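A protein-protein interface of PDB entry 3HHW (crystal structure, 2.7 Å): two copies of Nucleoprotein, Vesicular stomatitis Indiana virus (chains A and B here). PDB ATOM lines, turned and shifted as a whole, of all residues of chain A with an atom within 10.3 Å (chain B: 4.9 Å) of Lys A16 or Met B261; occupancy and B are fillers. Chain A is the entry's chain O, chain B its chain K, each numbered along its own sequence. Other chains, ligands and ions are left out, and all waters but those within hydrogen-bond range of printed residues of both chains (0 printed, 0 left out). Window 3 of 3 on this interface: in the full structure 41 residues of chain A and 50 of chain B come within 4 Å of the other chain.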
ATOM      1  N   SER A   1     -13.282 -23.702  -2.361  1.00  0.00           N
ATOM      2  CA  SER A   1     -13.315 -22.251  -2.000  1.00  0.00           C
ATOM      3  C   SER A   1     -14.746 -21.753  -1.763  1.00  0.00           C
ATOM      4  O   SER A   1     -15.717 -22.459  -2.057  1.00  0.00           O
ATOM      5  CB  SER A   1     -12.621 -21.409  -3.081  1.00  0.00           C
ATOM      6  OG  SER A   1     -13.231 -21.591  -4.349  1.00  0.00           O
ATOM      7  N   VAL A   2     -14.859 -20.535  -1.235  1.00  0.00           N
ATOM      8  CA  VAL A   2     -16.149 -19.928  -0.904  1.00  0.00           C
ATOM      9  C   VAL A   2     -16.784 -19.263  -2.130  1.00  0.00           C
ATOM     10  O   VAL A   2     -16.124 -18.516  -2.855  1.00  0.00           O
ATOM     11  CB  VAL A   2     -16.005 -18.892   0.245  1.00  0.00           C
ATOM     12  CG1 VAL A   2     -17.366 -18.388   0.697  1.00  0.00           C
ATOM     13  CG2 VAL A   2     -15.250 -19.493   1.426  1.00  0.00           C
ATOM     14  N   VAL A   4     -19.433 -16.626  -3.753  1.00  0.00           N
ATOM     15  CA  VAL A   4     -20.141 -15.370  -3.491  1.00  0.00           C
ATOM     16  C   VAL A   4     -21.079 -15.065  -4.650  1.00  0.00           C
ATOM     17  O   VAL A   4     -20.670 -15.105  -5.815  1.00  0.00           O
ATOM     18  CB  VAL A   4     -19.172 -14.166  -3.335  1.00  0.00           C
ATOM     19  CG1 VAL A   4     -19.911 -12.955  -2.787  1.00  0.00           C
ATOM     20  CG2 VAL A   4     -17.997 -14.517  -2.444  1.00  0.00           C
ATOM     21  N   VAL A  12     -22.864 -14.627 -10.062  1.00  0.00           N
ATOM     22  CA  VAL A  12     -21.705 -14.991  -9.247  1.00  0.00           C
ATOM     23  C   VAL A  12     -20.582 -13.963  -9.387  1.00  0.00           C
ATOM     24  O   VAL A  12     -20.217 -13.580 -10.501  1.00  0.00           O
ATOM     25  CB  VAL A  12     -21.179 -16.413  -9.599  1.00  0.00           C
ATOM     26  CG1 VAL A  12     -19.918 -16.754  -8.800  1.00  0.00           C
ATOM     27  CG2 VAL A  12     -22.258 -17.459  -9.354  1.00  0.00           C
ATOM     28  N   ILE A  13     -20.049 -13.518  -8.253  1.00  0.00           N
ATOM     29  CA  ILE A  13     -18.857 -12.673  -8.227  1.00  0.00           C
ATOM     30  C   ILE A  13     -17.713 -13.400  -7.509  1.00  0.00           C
ATOM     31  O   ILE A  13     -17.922 -14.056  -6.489  1.00  0.00           O
ATOM     32  CB  ILE A  13     -19.141 -11.265  -7.604  1.00  0.00           C
ATOM     33  CG1 ILE A  13     -17.909 -10.357  -7.708  1.00  0.00           C
ATOM     34  CG2 ILE A  13     -19.630 -11.378  -6.158  1.00  0.00           C
ATOM     35  CD1 ILE A  13     -18.200  -8.882  -7.516  1.00  0.00           C
ATOM     36  N   VAL A  14     -16.511 -13.296  -8.070  1.00  0.00           N
ATOM     37  CA  VAL A  14     -15.321 -13.911  -7.487  1.00  0.00           C
ATOM     38  C   VAL A  14     -14.346 -12.806  -7.051  1.00  0.00           C
ATOM     39  O   VAL A  14     -13.623 -12.252  -7.880  1.00  0.00           O
ATOM     40  CB  VAL A  14     -14.637 -14.900  -8.480  1.00  0.00           C
ATOM     41  CG1 VAL A  14     -13.528 -15.688  -7.794  1.00  0.00           C
ATOM     42  CG2 VAL A  14     -15.659 -15.855  -9.090  1.00  0.00           C
ATOM     43  N   PRO A  15     -14.339 -12.466  -5.748  1.00  0.00           N
ATOM     44  CA  PRO A  15     -13.440 -11.430  -5.230  1.00  0.00           C
ATOM     45  C   PRO A  15     -11.965 -11.810  -5.388  1.00  0.00           C
ATOM     46  O   PRO A  15     -11.527 -12.841  -4.875  1.00  0.00           O
ATOM     47  CB  PRO A  15     -13.824 -11.340  -3.745  1.00  0.00           C
ATOM     48  CG  PRO A  15     -15.194 -11.937  -3.668  1.00  0.00           C
ATOM     49  CD  PRO A  15     -15.191 -13.025  -4.685  1.00  0.00           C
ATOM     50  N   LYS A  16     -11.219 -10.973  -6.105  1.00  0.00           N
ATOM     51  CA  LYS A  16      -9.825 -11.249  -6.432  1.00  0.00           C
ATOM     52  C   LYS A  16      -8.924 -10.107  -6.001  1.00  0.00           C
ATOM     53  O   LYS A  16      -9.280  -8.935  -6.138  1.00  0.00           O
ATOM     54  CB  LYS A  16      -9.652 -11.452  -7.944  1.00  0.00           C
ATOM     55  CG  LYS A  16     -10.361 -12.659  -8.528  1.00  0.00           C
ATOM     56  CD  LYS A  16     -10.303 -12.659 -10.058  1.00  0.00           C
ATOM     57  CE  LYS A  16     -11.334 -11.708 -10.692  1.00  0.00           C
ATOM     58  NZ  LYS A  16     -12.753 -12.116 -10.430  1.00  0.00           N
ATOM     59  N   LEU A  17      -7.746 -10.469  -5.503  1.00  0.00           N
ATOM     60  CA  LEU A  17      -6.691  -9.521  -5.169  1.00  0.00           C
ATOM     61  C   LEU A  17      -5.366  -9.954  -5.787  1.00  0.00           C
ATOM     62  O   LEU A  17      -5.101 -11.154  -5.895  1.00  0.00           O
ATOM     63  CB  LEU A  17      -6.547  -9.399  -3.650  1.00  0.00           C
ATOM     64  CG  LEU A  17      -6.899  -8.090  -2.932  1.00  0.00           C
ATOM     65  CD1 LEU A  17      -7.982  -7.274  -3.624  1.00  0.00           C
ATOM     66  CD2 LEU A  17      -7.284  -8.391  -1.502  1.00  0.00           C
ATOM     67  N   PRO A  18      -4.532  -8.977  -6.200  1.00  0.00           N
ATOM     68  CA  PRO A  18      -3.208  -9.235  -6.764  1.00  0.00           C
ATOM     69  C   PRO A  18      -2.343 -10.135  -5.890  1.00  0.00           C
ATOM     70  O   PRO A  18      -2.245  -9.920  -4.686  1.00  0.00           O
ATOM     71  CB  PRO A  18      -2.596  -7.840  -6.843  1.00  0.00           C
ATOM     72  CG  PRO A  18      -3.756  -6.953  -7.031  1.00  0.00           C
ATOM     73  CD  PRO A  18      -4.829  -7.534  -6.170  1.00  0.00           C
ATOM     74  N   ALA A  19      -1.728 -11.137  -6.507  1.00  0.00           N
ATOM     75  CA  ALA A  19      -0.874 -12.092  -5.807  1.00  0.00           C
ATOM     76  C   ALA A  19       0.255 -11.402  -5.056  1.00  0.00           C
ATOM     77  O   ALA A  19       0.887 -10.478  -5.573  1.00  0.00           O
ATOM     78  CB  ALA A  19      -0.309 -13.113  -6.785  1.00  0.00           C
ATOM     79  N   ASN A  20       0.491 -11.850  -3.828  1.00  0.00           N
ATOM     80  CA  ASN A  20       1.624 -11.383  -3.034  1.00  0.00           C
ATOM     81  C   ASN A  20       2.392 -12.553  -2.411  1.00  0.00           C
ATOM     82  O   ASN A  20       2.140 -12.942  -1.260  1.00  0.00           O
ATOM     83  CB  ASN A  20       1.168 -10.385  -1.963  1.00  0.00           C
ATOM     84  CG  ASN A  20       2.336  -9.758  -1.210  1.00  0.00           C
ATOM     85  OD1 ASN A  20       3.457  -9.677  -1.725  1.00  0.00           O
ATOM     86  ND2 ASN A  20       2.073  -9.307   0.015  1.00  0.00           N
ATOM     87  N   LEU B 227      -7.857  -1.539  -6.454  1.00  0.00           N
ATOM     88  CA  LEU B 227      -7.429  -2.857  -5.965  1.00  0.00           C
ATOM     89  C   LEU B 227      -6.560  -2.746  -4.708  1.00  0.00           C
ATOM     90  O   LEU B 227      -6.504  -3.679  -3.892  1.00  0.00           O
ATOM     91  CB  LEU B 227      -6.702  -3.650  -7.051  1.00  0.00           C
ATOM     92  CG  LEU B 227      -7.495  -3.973  -8.323  1.00  0.00           C
ATOM     93  CD1 LEU B 227      -6.578  -4.536  -9.398  1.00  0.00           C
ATOM     94  CD2 LEU B 227      -8.656  -4.919  -8.059  1.00  0.00           C
ATOM     95  N   PHE B 230      -9.083  -2.030  -1.749  1.00  0.00           N
ATOM     96  CA  PHE B 230      -9.668  -3.325  -1.417  1.00  0.00           C
ATOM     97  C   PHE B 230      -8.699  -4.161  -0.575  1.00  0.00           C
ATOM     98  O   PHE B 230      -9.070  -4.677   0.480  1.00  0.00           O
ATOM     99  CB  PHE B 230     -10.057  -4.049  -2.719  1.00  0.00           C
ATOM    100  CG  PHE B 230     -10.985  -5.229  -2.534  1.00  0.00           C
ATOM    101  CD1 PHE B 230     -11.686  -5.427  -1.358  1.00  0.00           C
ATOM    102  CD2 PHE B 230     -11.185  -6.127  -3.587  1.00  0.00           C
ATOM    103  CE1 PHE B 230     -12.546  -6.518  -1.216  1.00  0.00           C
ATOM    104  CE2 PHE B 230     -12.047  -7.221  -3.453  1.00  0.00           C
ATOM    105  CZ  PHE B 230     -12.726  -7.412  -2.267  1.00  0.00           C
ATOM    106  N   MET B 257     -17.839  -2.769  -7.443  1.00  0.00           N
ATOM    107  CA  MET B 257     -17.152  -4.014  -7.113  1.00  0.00           C
ATOM    108  C   MET B 257     -17.280  -5.084  -8.217  1.00  0.00           C
ATOM    109  O   MET B 257     -16.320  -5.821  -8.470  1.00  0.00           O
ATOM    110  CB  MET B 257     -17.627  -4.552  -5.759  1.00  0.00           C
ATOM    111  CG  MET B 257     -16.870  -5.779  -5.255  1.00  0.00           C
ATOM    112  SD  MET B 257     -15.080  -5.561  -5.249  1.00  0.00           S
ATOM    113  CE  MET B 257     -14.839  -4.693  -3.701  1.00  0.00           C
ATOM    114  N   VAL B 258     -18.438  -5.168  -8.878  1.00  0.00           N
ATOM    115  CA  VAL B 258     -18.580  -6.121  -9.987  1.00  0.00           C
ATOM    116  C   VAL B 258     -17.718  -5.705 -11.187  1.00  0.00           C
ATOM    117  O   VAL B 258     -17.078  -6.548 -11.813  1.00  0.00           O
ATOM    118  CB  VAL B 258     -20.069  -6.433 -10.401  1.00  0.00           C
ATOM    119  CG1 VAL B 258     -20.920  -6.781  -9.183  1.00  0.00           C
ATOM    120  CG2 VAL B 258     -20.704  -5.296 -11.196  1.00  0.00           C
ATOM    121  N   GLN B 259     -17.696  -4.404 -11.477  1.00  0.00           N
ATOM    122  CA  GLN B 259     -16.858  -3.834 -12.530  1.00  0.00           C
ATOM    123  C   GLN B 259     -15.382  -4.129 -12.264  1.00  0.00           C
ATOM    124  O   GLN B 259     -14.643  -4.501 -13.171  1.00  0.00           O
ATOM    125  CB  GLN B 259     -17.092  -2.322 -12.622  1.00  0.00           C
ATOM    126  CG  GLN B 259     -16.416  -1.642 -13.801  1.00  0.00           C
ATOM    127  CD  GLN B 259     -16.481  -0.124 -13.729  1.00  0.00           C
ATOM    128  OE1 GLN B 259     -16.028   0.488 -12.757  1.00  0.00           O
ATOM    129  NE2 GLN B 259     -17.031   0.491 -14.771  1.00  0.00           N
ATOM    130  N   MET B 260     -14.975  -3.975 -11.008  1.00  0.00           N
ATOM    131  CA  MET B 260     -13.598  -4.214 -10.569  1.00  0.00           C
ATOM    132  C   MET B 260     -13.172  -5.681 -10.648  1.00  0.00           C
ATOM    133  O   MET B 260     -11.984  -5.977 -10.780  1.00  0.00           O
ATOM    134  CB  MET B 260     -13.417  -3.717  -9.131  1.00  0.00           C
ATOM    135  CG  MET B 260     -13.241  -2.214  -8.996  1.00  0.00           C
ATOM    136  SD  MET B 260     -13.344  -1.638  -7.289  1.00  0.00           S
ATOM    137  CE  MET B 260     -11.988  -2.537  -6.527  1.00  0.00           C
ATOM    138  N   MET B 261     -14.142  -6.588 -10.560  1.00  0.00           N
ATOM    139  CA  MET B 261     -13.852  -8.019 -10.448  1.00  0.00           C
ATOM    140  C   MET B 261     -14.181  -8.829 -11.703  1.00  0.00           C
ATOM    141  O   MET B 261     -14.174 -10.065 -11.661  1.00  0.00           O
ATOM    142  CB  MET B 261     -14.585  -8.616  -9.239  1.00  0.00           C
ATOM    143  CG  MET B 261     -14.065  -8.174  -7.874  1.00  0.00           C
ATOM    144  SD  MET B 261     -12.318  -8.520  -7.601  1.00  0.00           S
ATOM    145  CE  MET B 261     -11.640  -6.867  -7.621  1.00  0.00           C
ATOM    146  N   LEU B 262     -14.459  -8.142 -12.814  1.00  0.00           N
ATOM    147  CA  LEU B 262     -14.793  -8.810 -14.072  1.00  0.00           C
ATOM    148  C   LEU B 262     -13.757  -9.895 -14.390  1.00  0.00           C
ATOM    149  O   LEU B 262     -12.555  -9.630 -14.350  1.00  0.00           O
ATOM    150  CB  LEU B 262     -14.891  -7.796 -15.215  1.00  0.00           C
ATOM    151  CG  LEU B 262     -15.718  -8.226 -16.434  1.00  0.00           C
ATOM    152  CD1 LEU B 262     -17.217  -8.138 -16.141  1.00  0.00           C
ATOM    153  CD2 LEU B 262     -15.368  -7.401 -17.659  1.00  0.00           C
ATOM    154  N   PRO B 263     -14.220 -11.127 -14.680  1.00  0.00           N
ATOM    155  CA  PRO B 263     -13.305 -12.259 -14.852  1.00  0.00           C
ATOM    156  C   PRO B 263     -12.391 -12.121 -16.071  1.00  0.00           C
ATOM    157  O   PRO B 263     -12.697 -11.364 -16.996  1.00  0.00           O
ATOM    158  CB  PRO B 263     -14.254 -13.450 -15.034  1.00  0.00           C
ATOM    159  CG  PRO B 263     -15.572 -12.989 -14.516  1.00  0.00           C
ATOM    160  CD  PRO B 263     -15.622 -11.544 -14.855  1.00  0.00           C
ATOM    161  N   ILE B 267      -5.791 -10.622 -12.685  1.00  0.00           N
ATOM    162  CA  ILE B 267      -5.509  -9.877 -11.455  1.00  0.00           C
ATOM    163  C   ILE B 267      -4.558 -10.651 -10.547  1.00  0.00           C
ATOM    164  O   ILE B 267      -3.537 -10.112 -10.100  1.00  0.00           O
ATOM    165  CB  ILE B 267      -6.802  -9.542 -10.640  1.00  0.00           C
ATOM    166  CG1 ILE B 267      -7.910  -8.947 -11.525  1.00  0.00           C
ATOM    167  CG2 ILE B 267      -6.473  -8.640  -9.438  1.00  0.00           C
ATOM    168  CD1 ILE B 267      -7.742  -7.483 -11.882  1.00  0.00           C
ATOM    169  N   ASP B 268      -4.893 -11.914 -10.285  1.00  0.00           N
ATOM    170  CA  ASP B 268      -4.173 -12.713  -9.294  1.00  0.00           C
ATOM    171  C   ASP B 268      -3.037 -13.556  -9.874  1.00  0.00           C
ATOM    172  O   ASP B 268      -2.442 -14.376  -9.173  1.00  0.00           O
ATOM    173  CB  ASP B 268      -5.143 -13.587  -8.479  1.00  0.00           C
ATOM    174  CG  ASP B 268      -6.048 -14.452  -9.350  1.00  0.00           C
ATOM    175  OD1 ASP B 268      -6.985 -15.059  -8.788  1.00  0.00           O
ATOM    176  OD2 ASP B 268      -5.834 -14.522 -10.583  1.00  0.00           O
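The backbone carbonyl oxygen (O) of Met B261 sits at hydrogen-bond distance from the side-chain amino group (NZ) of Lys A16.
The backbone carbonyl oxygen of Val A4 is in hydrogen-bond range of the backbone NH of Ile A13, at 3.0 Å.
The backbone carbonyl oxygen (O) of Val A14 lies within hydrogen-bond range of the side-chain amino group (NZ) of Lys A16 (2.7 Å).
Of the printed residues of chain A, Met B261 touches Val A14 (3.96 Å), Pro A15 (3.9 Å) and Lys A16 (2.8 Å).
Printed residues of chain A within 4 Å of Met B257: Ile A13.
No residue of chain A comes within 4 Å of Leu B262.
No residue of chain A comes within 4 Å of Pro B263.
Printed residues of chain A within 4 Å of Phe B230: Leu A17 (3.4 Å).
Printed residues of chain B within 4 Å of Val A14: Met B261.
The nearest residue of chain B that does not touch Lys A16 is Asp B268 (4.2 Å).
The nearest printed residue of chain B that does not touch Pro A18 is Leu B227 (4.4 Å).
Of the 11 printed residues of chain B, 7 touch a printed residue of chain A.
Hydrophobic or aromatic side chains of chain B that line the printed part of chain A: Phe B230, Val B258, Met B261 and Ile B267.
Printed residues of chain A that touch a printed residue of chain B: Ile A13, Val A14, Pro A15, Lys A16, Leu A17, Pro A18 and Ala A19.
Among the printed residues, no Asp or Glu carboxylate lies within 4 Å of a Lys or Arg side-chain nitrogen of the other chain.
Among the printed residues, pairs that only touch across the chains: Ile A13 with Met B257, Ile A13 with Val B258, Val A14 with Met B261, Pro A15 with Met B261, Leu A17 with Leu B227, Leu A17 with Phe B230, Leu A17 with Asp B268, Pro A18 with Ile B267 and Ala A19 with Asp B268.
No position is printed for both chains.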
